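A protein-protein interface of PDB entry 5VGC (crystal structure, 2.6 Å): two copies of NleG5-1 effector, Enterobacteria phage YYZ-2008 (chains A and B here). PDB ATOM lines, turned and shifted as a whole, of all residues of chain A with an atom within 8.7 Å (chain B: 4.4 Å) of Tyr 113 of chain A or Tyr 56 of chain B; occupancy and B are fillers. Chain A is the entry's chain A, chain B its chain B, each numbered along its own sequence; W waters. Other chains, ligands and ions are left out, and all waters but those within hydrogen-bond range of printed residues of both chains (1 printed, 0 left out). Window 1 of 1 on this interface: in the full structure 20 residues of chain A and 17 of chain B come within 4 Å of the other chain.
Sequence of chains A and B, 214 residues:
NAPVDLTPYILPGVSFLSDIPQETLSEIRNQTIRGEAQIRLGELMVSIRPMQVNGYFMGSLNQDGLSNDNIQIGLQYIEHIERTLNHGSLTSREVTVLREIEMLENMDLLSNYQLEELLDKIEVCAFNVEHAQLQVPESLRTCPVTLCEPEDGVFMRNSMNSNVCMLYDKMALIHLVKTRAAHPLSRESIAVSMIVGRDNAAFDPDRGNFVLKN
OH of Tyr 56 of chain B sits at hydrogen-bond distance from O of Leu 110 of chain A (3.4 Å). The side-chain hydroxyl (OH) of Tyr 56 of chain B lies close to the side-chain amide nitrogen (NE2) of Gln 114 of chain A.
Among the printed residues, merely in contact across the chains: Met 107 of chain A with Val 53 of chain B (3.6 Å), Leu 110 of chain A with Leu 98 of chain B (3.6 Å), Tyr 113 of chain A with Tyr 56 of chain B (3.97 Å), Tyr 113 of chain A with His 87 of chain B (3.9 Å), Tyr 113 of chain A with Gly 88 of chain B (3.7 Å), Tyr 113 of chain A with Leu 98 of chain B (3.8 Å), Gln 114 of chain A with Asn 54 of chain B (3.6 Å), Gln 114 of chain A with His 87 of chain B (3.7 Å) and Glu 117 of chain A with His 87 of chain B (3.4 Å).
O of Gly 55 of chain B lies close to NE2 of His 87 of chain B. The backbone carbonyl oxygen (O) of Tyr 56 of chain B sits at hydrogen-bond distance from the backbone NH (N) of Met 51 of chain B, at 2.8 Å. O of Met 107 of chain A sits close to OG of Ser 111 of chain A (3.1 Å).
Water W1 lies within hydrogen-bond range of OE1 of Glu 117 of chain A (2.7 Å), ND1 of His 87 of chain B (2.9 Å) and O of Tyr 113 of chain A (3.3 Å).
Of chain B, only Tyr 56, His 87, Gly 88 and Leu 98 come within 4 Å of Tyr 113 of chain A. Of the printed residues of chain B, Gln 114 of chain A touches Asn 54 (3.6 Å), Tyr 56 (3.1 Å) and His 87 (3.7 Å). Printed residues of chain A within 4 Å of Val 53 of chain B: Met 107. No residue of chain A comes within 4 Å of Gly 55 of chain B. Tyr 56 of chain B touches three residues of chain A. Gly 88 of chain B touches one residue of chain A. Val 95 of chain B touches none of the printed residues of chain A.
Printed residues of chain A that touch a printed residue of chain B: Met 107, Leu 110, Tyr 113, Gln 114 and Glu 117. Of the 13 printed residues of chain B, 6 touch a printed residue of chain A. Hydrophobic or aromatic side chains of chain B that line the printed part of chain A: Val 53, Tyr 56, His 87 and Leu 98. Among the printed residues, 11 pairs touch across the chains.
No position is printed for both chains.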
ATOM      1  N   MET A 107     -21.247  11.914 -33.749  1.00  0.00           N
ATOM      2  CA  MET A 107     -20.362  10.740 -33.625  1.00  0.00           C
ATOM      3  C   MET A 107     -19.922  10.027 -34.909  1.00  0.00           C
ATOM      4  O   MET A 107     -19.139   9.075 -34.806  1.00  0.00           O
ATOM      5  CB  MET A 107     -20.937   9.713 -32.623  1.00  0.00           C
ATOM      6  CG  MET A 107     -21.198  10.262 -31.233  1.00  0.00           C
ATOM      7  SD  MET A 107     -19.685  10.798 -30.386  1.00  0.00           S
ATOM      8  CE  MET A 107     -18.684   9.338 -30.613  1.00  0.00           C
ATOM      9  N   ASP A 108     -20.367  10.473 -36.098  1.00  0.00           N
ATOM     10  CA  ASP A 108     -20.008   9.739 -37.341  1.00  0.00           C
ATOM     11  C   ASP A 108     -18.495   9.757 -37.613  1.00  0.00           C
ATOM     12  O   ASP A 108     -17.949   8.767 -38.112  1.00  0.00           O
ATOM     13  CB  ASP A 108     -20.738  10.292 -38.579  1.00  0.00           C
ATOM     14  CG  ASP A 108     -22.011   9.519 -38.949  1.00  0.00           C
ATOM     15  OD1 ASP A 108     -22.197   8.362 -38.511  1.00  0.00           O
ATOM     16  OD2 ASP A 108     -22.828  10.072 -39.734  1.00  0.00           O
ATOM     17  N   LEU A 109     -17.832  10.870 -37.287  1.00  0.00           N
ATOM     18  CA  LEU A 109     -16.385  10.969 -37.407  1.00  0.00           C
ATOM     19  C   LEU A 109     -15.693  10.474 -36.158  1.00  0.00           C
ATOM     20  O   LEU A 109     -14.718   9.754 -36.284  1.00  0.00           O
ATOM     21  CB  LEU A 109     -15.950  12.409 -37.728  1.00  0.00           C
ATOM     22  CG  LEU A 109     -16.458  13.001 -39.056  1.00  0.00           C
ATOM     23  CD1 LEU A 109     -15.850  14.373 -39.299  1.00  0.00           C
ATOM     24  CD2 LEU A 109     -16.160  12.123 -40.254  1.00  0.00           C
ATOM     25  N   LEU A 110     -16.169  10.829 -34.974  1.00  0.00           N
ATOM     26  CA  LEU A 110     -15.522  10.343 -33.741  1.00  0.00           C
ATOM     27  C   LEU A 110     -15.686   8.851 -33.401  1.00  0.00           C
ATOM     28  O   LEU A 110     -14.934   8.361 -32.555  1.00  0.00           O
ATOM     29  CB  LEU A 110     -15.929  11.184 -32.538  1.00  0.00           C
ATOM     30  CG  LEU A 110     -15.435  12.622 -32.617  1.00  0.00           C
ATOM     31  CD1 LEU A 110     -16.134  13.473 -31.559  1.00  0.00           C
ATOM     32  CD2 LEU A 110     -13.921  12.686 -32.433  1.00  0.00           C
ATOM     33  N   SER A 111     -16.610   8.136 -34.051  1.00  0.00           N
ATOM     34  CA  SER A 111     -16.751   6.693 -33.803  1.00  0.00           C
ATOM     35  C   SER A 111     -15.516   5.858 -34.241  1.00  0.00           C
ATOM     36  O   SER A 111     -15.090   4.907 -33.500  1.00  0.00           O
ATOM     37  CB  SER A 111     -18.040   6.173 -34.437  1.00  0.00           C
ATOM     38  OG  SER A 111     -18.046   6.332 -35.847  1.00  0.00           O
ATOM     39  N   ASN A 112     -14.905   6.227 -35.384  1.00  0.00           N
ATOM     40  CA  ASN A 112     -13.682   5.581 -35.889  1.00  0.00           C
ATOM     41  C   ASN A 112     -12.605   5.390 -34.811  1.00  0.00           C
ATOM     42  O   ASN A 112     -11.885   4.395 -34.806  1.00  0.00           O
ATOM     43  CB  ASN A 112     -13.042   6.369 -37.050  1.00  0.00           C
ATOM     44  CG  ASN A 112     -13.963   6.527 -38.267  1.00  0.00           C
ATOM     45  OD1 ASN A 112     -15.199   6.513 -38.183  1.00  0.00           O
ATOM     46  ND2 ASN A 112     -13.348   6.694 -39.410  1.00  0.00           N
ATOM     47  N   TYR A 113     -12.488   6.362 -33.916  1.00  0.00           N
ATOM     48  CA  TYR A 113     -11.461   6.309 -32.887  1.00  0.00           C
ATOM     49  C   TYR A 113     -11.875   5.416 -31.719  1.00  0.00           C
ATOM     50  O   TYR A 113     -11.051   4.822 -31.037  1.00  0.00           O
ATOM     51  CB  TYR A 113     -11.088   7.748 -32.483  1.00  0.00           C
ATOM     52  CG  TYR A 113     -10.678   8.558 -33.724  1.00  0.00           C
ATOM     53  CD1 TYR A 113      -9.390   8.470 -34.249  1.00  0.00           C
ATOM     54  CD2 TYR A 113     -11.597   9.384 -34.386  1.00  0.00           C
ATOM     55  CE1 TYR A 113      -9.024   9.181 -35.372  1.00  0.00           C
ATOM     56  CE2 TYR A 113     -11.244  10.097 -35.514  1.00  0.00           C
ATOM     57  CZ  TYR A 113      -9.954   9.998 -36.005  1.00  0.00           C
ATOM     58  OH  TYR A 113      -9.587  10.709 -37.129  1.00  0.00           O
ATOM     59  N   GLN A 114     -13.187   5.331 -31.477  1.00  0.00           N
ATOM     60  CA  GLN A 114     -13.747   4.571 -30.331  1.00  0.00           C
ATOM     61  C   GLN A 114     -14.051   3.071 -30.665  1.00  0.00           C
ATOM     62  O   GLN A 114     -14.279   2.211 -29.768  1.00  0.00           O
ATOM     63  CB  GLN A 114     -15.052   5.243 -29.945  1.00  0.00           C
ATOM     64  CG  GLN A 114     -14.904   6.664 -29.445  1.00  0.00           C
ATOM     65  CD  GLN A 114     -16.224   7.324 -29.136  1.00  0.00           C
ATOM     66  OE1 GLN A 114     -17.298   6.778 -29.424  1.00  0.00           O
ATOM     67  NE2 GLN A 114     -16.159   8.508 -28.539  1.00  0.00           N
ATOM     68  N   LEU A 115     -14.070   2.796 -31.958  1.00  0.00           N
ATOM     69  CA  LEU A 115     -14.613   1.538 -32.445  1.00  0.00           C
ATOM     70  C   LEU A 115     -13.917   0.278 -31.905  1.00  0.00           C
ATOM     71  O   LEU A 115     -14.580  -0.659 -31.412  1.00  0.00           O
ATOM     72  CB  LEU A 115     -14.606   1.503 -33.981  1.00  0.00           C
ATOM     73  CG  LEU A 115     -15.416   0.404 -34.622  1.00  0.00           C
ATOM     74  CD1 LEU A 115     -16.913   0.633 -34.421  1.00  0.00           C
ATOM     75  CD2 LEU A 115     -15.096   0.328 -36.106  1.00  0.00           C
ATOM     76  N   GLU A 116     -12.583   0.264 -32.021  1.00  0.00           N
ATOM     77  CA  GLU A 116     -11.768  -0.907 -31.664  1.00  0.00           C
ATOM     78  C   GLU A 116     -11.901  -1.243 -30.168  1.00  0.00           C
ATOM     79  O   GLU A 116     -12.132  -2.408 -29.810  1.00  0.00           O
ATOM     80  CB  GLU A 116     -10.298  -0.715 -32.082  1.00  0.00           C
ATOM     81  CG  GLU A 116      -9.909  -1.396 -33.390  1.00  0.00           C
ATOM     82  CD  GLU A 116      -9.135  -2.693 -33.161  1.00  0.00           C
ATOM     83  OE1 GLU A 116      -9.688  -3.605 -32.507  1.00  0.00           O
ATOM     84  OE2 GLU A 116      -7.974  -2.801 -33.626  1.00  0.00           O
ATOM     85  N   GLU A 117     -11.781  -0.218 -29.329  1.00  0.00           N
ATOM     86  CA  GLU A 117     -12.064  -0.312 -27.901  1.00  0.00           C
ATOM     87  C   GLU A 117     -13.475  -0.893 -27.594  1.00  0.00           C
ATOM     88  O   GLU A 117     -13.632  -1.819 -26.762  1.00  0.00           O
ATOM     89  CB  GLU A 117     -11.850   1.071 -27.260  1.00  0.00           C
ATOM     90  CG  GLU A 117     -12.381   1.257 -25.837  1.00  0.00           C
ATOM     91  CD  GLU A 117     -11.691   2.343 -25.030  1.00  0.00           C
ATOM     92  OE1 GLU A 117     -10.592   2.781 -25.434  1.00  0.00           O
ATOM     93  OE2 GLU A 117     -12.258   2.736 -23.984  1.00  0.00           O
ATOM     94  N   LEU A 118     -14.485  -0.369 -28.277  1.00  0.00           N
ATOM     95  CA  LEU A 118     -15.864  -0.806 -28.081  1.00  0.00           C
ATOM     96  C   LEU A 118     -16.062  -2.293 -28.482  1.00  0.00           C
ATOM     97  O   LEU A 118     -16.658  -3.112 -27.720  1.00  0.00           O
ATOM     98  CB  LEU A 118     -16.801   0.113 -28.868  1.00  0.00           C
ATOM     99  CG  LEU A 118     -18.302  -0.054 -28.760  1.00  0.00           C
ATOM    100  CD1 LEU A 118     -18.746  -0.079 -27.313  1.00  0.00           C
ATOM    101  CD2 LEU A 118     -18.937   1.118 -29.483  1.00  0.00           C
ATOM    102  N   ARG A 180     -22.920   2.242 -36.514  1.00  0.00           N
ATOM    103  CA  ARG A 180     -23.128   3.489 -35.767  1.00  0.00           C
ATOM    104  C   ARG A 180     -24.629   3.732 -35.453  1.00  0.00           C
ATOM    105  O   ARG A 180     -25.085   4.885 -35.349  1.00  0.00           O
ATOM    106  CB  ARG A 180     -22.512   4.691 -36.543  1.00  0.00           C
ATOM    107  CG  ARG A 180     -20.997   4.827 -36.442  1.00  0.00           C
ATOM    108  CD  ARG A 180     -20.236   3.819 -37.294  1.00  0.00           C
ATOM    109  NE  ARG A 180     -18.788   4.080 -37.268  1.00  0.00           N
ATOM    110  CZ  ARG A 180     -17.868   3.360 -37.917  1.00  0.00           C
ATOM    111  NH1 ARG A 180     -18.225   2.306 -38.649  1.00  0.00           N
ATOM    112  NH2 ARG A 180     -16.581   3.689 -37.830  1.00  0.00           N
ATOM    113  N   PRO B  50     -14.118  16.711 -18.243  1.00  0.00           N
ATOM    114  CA  PRO B  50     -14.671  15.882 -19.308  1.00  0.00           C
ATOM    115  C   PRO B  50     -15.268  16.773 -20.387  1.00  0.00           C
ATOM    116  O   PRO B  50     -15.955  17.744 -20.059  1.00  0.00           O
ATOM    117  CB  PRO B  50     -15.756  15.072 -18.602  1.00  0.00           C
ATOM    118  CG  PRO B  50     -16.207  15.953 -17.494  1.00  0.00           C
ATOM    119  CD  PRO B  50     -15.014  16.764 -17.068  1.00  0.00           C
ATOM    120  N   MET B  51     -15.004  16.455 -21.656  1.00  0.00           N
ATOM    121  CA  MET B  51     -15.517  17.256 -22.765  1.00  0.00           C
ATOM    122  C   MET B  51     -16.998  16.983 -22.967  1.00  0.00           C
ATOM    123  O   MET B  51     -17.561  16.046 -22.389  1.00  0.00           O
ATOM    124  CB  MET B  51     -14.753  16.960 -24.066  1.00  0.00           C
ATOM    125  CG  MET B  51     -13.323  17.432 -24.061  1.00  0.00           C
ATOM    126  SD  MET B  51     -12.493  17.262 -25.654  1.00  0.00           S
ATOM    127  CE  MET B  51     -13.224  18.620 -26.554  1.00  0.00           C
ATOM    128  N   VAL B  53     -18.434  15.805 -25.463  1.00  0.00           N
ATOM    129  CA  VAL B  53     -18.572  14.463 -26.033  1.00  0.00           C
ATOM    130  C   VAL B  53     -18.136  13.438 -24.992  1.00  0.00           C
ATOM    131  O   VAL B  53     -17.165  13.664 -24.266  1.00  0.00           O
ATOM    132  CB  VAL B  53     -17.683  14.235 -27.274  1.00  0.00           C
ATOM    133  CG1 VAL B  53     -18.102  12.932 -27.957  1.00  0.00           C
ATOM    134  CG2 VAL B  53     -17.700  15.427 -28.228  1.00  0.00           C
ATOM    135  N   ASN B  54     -18.840  12.313 -24.933  1.00  0.00           N
ATOM    136  CA  ASN B  54     -18.538  11.264 -23.963  1.00  0.00           C
ATOM    137  C   ASN B  54     -17.227  10.575 -24.337  1.00  0.00           C
ATOM    138  O   ASN B  54     -16.992  10.257 -25.511  1.00  0.00           O
ATOM    139  CB  ASN B  54     -19.675  10.231 -23.890  1.00  0.00           C
ATOM    140  CG  ASN B  54     -19.598   9.352 -22.645  1.00  0.00           C
ATOM    141  OD1 ASN B  54     -19.133   9.781 -21.585  1.00  0.00           O
ATOM    142  ND2 ASN B  54     -20.064   8.111 -22.770  1.00  0.00           N
ATOM    143  N   GLY B  55     -16.377  10.360 -23.333  1.00  0.00           N
ATOM    144  CA  GLY B  55     -15.128   9.606 -23.510  1.00  0.00           C
ATOM    145  C   GLY B  55     -13.903  10.453 -23.790  1.00  0.00           C
ATOM    146  O   GLY B  55     -12.793   9.912 -23.892  1.00  0.00           O
ATOM    147  N   TYR B  56     -14.081  11.771 -23.918  1.00  0.00           N
ATOM    148  CA  TYR B  56     -12.979  12.663 -24.228  1.00  0.00           C
ATOM    149  C   TYR B  56     -12.780  13.674 -23.117  1.00  0.00           C
ATOM    150  O   TYR B  56     -13.734  14.087 -22.447  1.00  0.00           O
ATOM    151  CB  TYR B  56     -13.210  13.368 -25.555  1.00  0.00           C
ATOM    152  CG  TYR B  56     -13.225  12.434 -26.731  1.00  0.00           C
ATOM    153  CD1 TYR B  56     -14.425  11.963 -27.240  1.00  0.00           C
ATOM    154  CD2 TYR B  56     -12.044  12.012 -27.333  1.00  0.00           C
ATOM    155  CE1 TYR B  56     -14.453  11.102 -28.318  1.00  0.00           C
ATOM    156  CE2 TYR B  56     -12.065  11.153 -28.415  1.00  0.00           C
ATOM    157  CZ  TYR B  56     -13.276  10.705 -28.901  1.00  0.00           C
ATOM    158  OH  TYR B  56     -13.324   9.855 -29.966  1.00  0.00           O
ATOM    159  N   PHE B  57     -11.522  14.070 -22.943  1.00  0.00           N
ATOM    160  CA  PHE B  57     -11.103  14.868 -21.806  1.00  0.00           C
ATOM    161  C   PHE B  57     -10.276  16.043 -22.290  1.00  0.00           C
ATOM    162  O   PHE B  57      -9.577  15.960 -23.316  1.00  0.00           O
ATOM    163  CB  PHE B  57     -10.310  14.005 -20.819  1.00  0.00           C
ATOM    164  CG  PHE B  57     -11.059  12.791 -20.366  1.00  0.00           C
ATOM    165  CD1 PHE B  57     -11.961  12.873 -19.313  1.00  0.00           C
ATOM    166  CD2 PHE B  57     -10.888  11.569 -21.002  1.00  0.00           C
ATOM    167  CE1 PHE B  57     -12.674  11.755 -18.890  1.00  0.00           C
ATOM    168  CE2 PHE B  57     -11.595  10.441 -20.584  1.00  0.00           C
ATOM    169  CZ  PHE B  57     -12.492  10.537 -19.529  1.00  0.00           C
ATOM    170  N   ASN B  86      -7.463  10.341 -24.294  1.00  0.00           N
ATOM    171  CA  ASN B  86      -8.527  10.351 -25.312  1.00  0.00           C
ATOM    172  C   ASN B  86      -8.508   9.173 -26.283  1.00  0.00           C
ATOM    173  O   ASN B  86      -7.464   8.571 -26.524  1.00  0.00           O
ATOM    174  CB  ASN B  86      -8.488  11.660 -26.099  1.00  0.00           C
ATOM    175  CG  ASN B  86      -8.894  12.870 -25.261  1.00  0.00           C
ATOM    176  OD1 ASN B  86      -9.528  12.748 -24.198  1.00  0.00           O
ATOM    177  ND2 ASN B  86      -8.518  14.047 -25.733  1.00  0.00           N
ATOM    178  N   HIS B  87      -9.685   8.860 -26.841  1.00  0.00           N
ATOM    179  CA  HIS B  87      -9.807   7.854 -27.893  1.00  0.00           C
ATOM    180  C   HIS B  87      -9.119   8.372 -29.159  1.00  0.00           C
ATOM    181  O   HIS B  87      -9.223   9.557 -29.477  1.00  0.00           O
ATOM    182  CB  HIS B  87     -11.269   7.551 -28.227  1.00  0.00           C
ATOM    183  CG  HIS B  87     -12.087   7.084 -27.067  1.00  0.00           C
ATOM    184  ND1 HIS B  87     -12.180   5.756 -26.723  1.00  0.00           N
ATOM    185  CD2 HIS B  87     -12.861   7.761 -26.178  1.00  0.00           C
ATOM    186  CE1 HIS B  87     -12.969   5.630 -25.669  1.00  0.00           C
ATOM    187  NE2 HIS B  87     -13.392   6.831 -25.317  1.00  0.00           N
ATOM    188  N   GLY B  88      -8.428   7.482 -29.868  1.00  0.00           N
ATOM    189  CA  GLY B  88      -7.651   7.847 -31.055  1.00  0.00           C
ATOM    190  C   GLY B  88      -6.380   8.640 -30.784  1.00  0.00           C
ATOM    191  O   GLY B  88      -5.763   9.143 -31.721  1.00  0.00           O
ATOM    192  N   LEU B  90      -6.168  11.546 -29.615  1.00  0.00           N
ATOM    193  CA  LEU B  90      -6.466  12.896 -30.067  1.00  0.00           C
ATOM    194  C   LEU B  90      -6.314  13.926 -28.952  1.00  0.00           C
ATOM    195  O   LEU B  90      -6.610  13.641 -27.795  1.00  0.00           O
ATOM    196  CB  LEU B  90      -7.905  12.970 -30.584  1.00  0.00           C
ATOM    197  CG  LEU B  90      -8.303  12.019 -31.718  1.00  0.00           C
ATOM    198  CD1 LEU B  90      -9.816  12.096 -31.962  1.00  0.00           C
ATOM    199  CD2 LEU B  90      -7.542  12.312 -33.004  1.00  0.00           C
ATOM    200  N   VAL B  95     -10.482  16.935 -31.414  1.00  0.00           N
ATOM    201  CA  VAL B  95     -11.832  16.488 -31.077  1.00  0.00           C
ATOM    202  C   VAL B  95     -12.841  17.589 -31.448  1.00  0.00           C
ATOM    203  O   VAL B  95     -13.795  17.350 -32.200  1.00  0.00           O
ATOM    204  CB  VAL B  95     -11.943  16.101 -29.578  1.00  0.00           C
ATOM    205  CG1 VAL B  95     -13.392  15.784 -29.197  1.00  0.00           C
ATOM    206  CG2 VAL B  95     -11.042  14.900 -29.274  1.00  0.00           C
ATOM    207  N   LEU B  98     -13.225  17.920 -35.175  1.00  0.00           N
ATOM    208  CA  LEU B  98     -14.065  16.852 -35.734  1.00  0.00           C
ATOM    209  C   LEU B  98     -15.570  17.066 -35.399  1.00  0.00           C
ATOM    210  O   LEU B  98     -16.488  16.931 -36.267  1.00  0.00           O
ATOM    211  CB  LEU B  98     -13.584  15.504 -35.257  1.00  0.00           C
ATOM    212  CG  LEU B  98     -12.218  15.065 -35.781  1.00  0.00           C
ATOM    213  CD1 LEU B  98     -11.731  13.805 -35.059  1.00  0.00           C
ATOM    214  CD2 LEU B  98     -12.285  14.827 -37.280  1.00  0.00           C
HETATM  215  O   HOH W   1     -10.479   3.745 -27.945  1.00  0.00           O
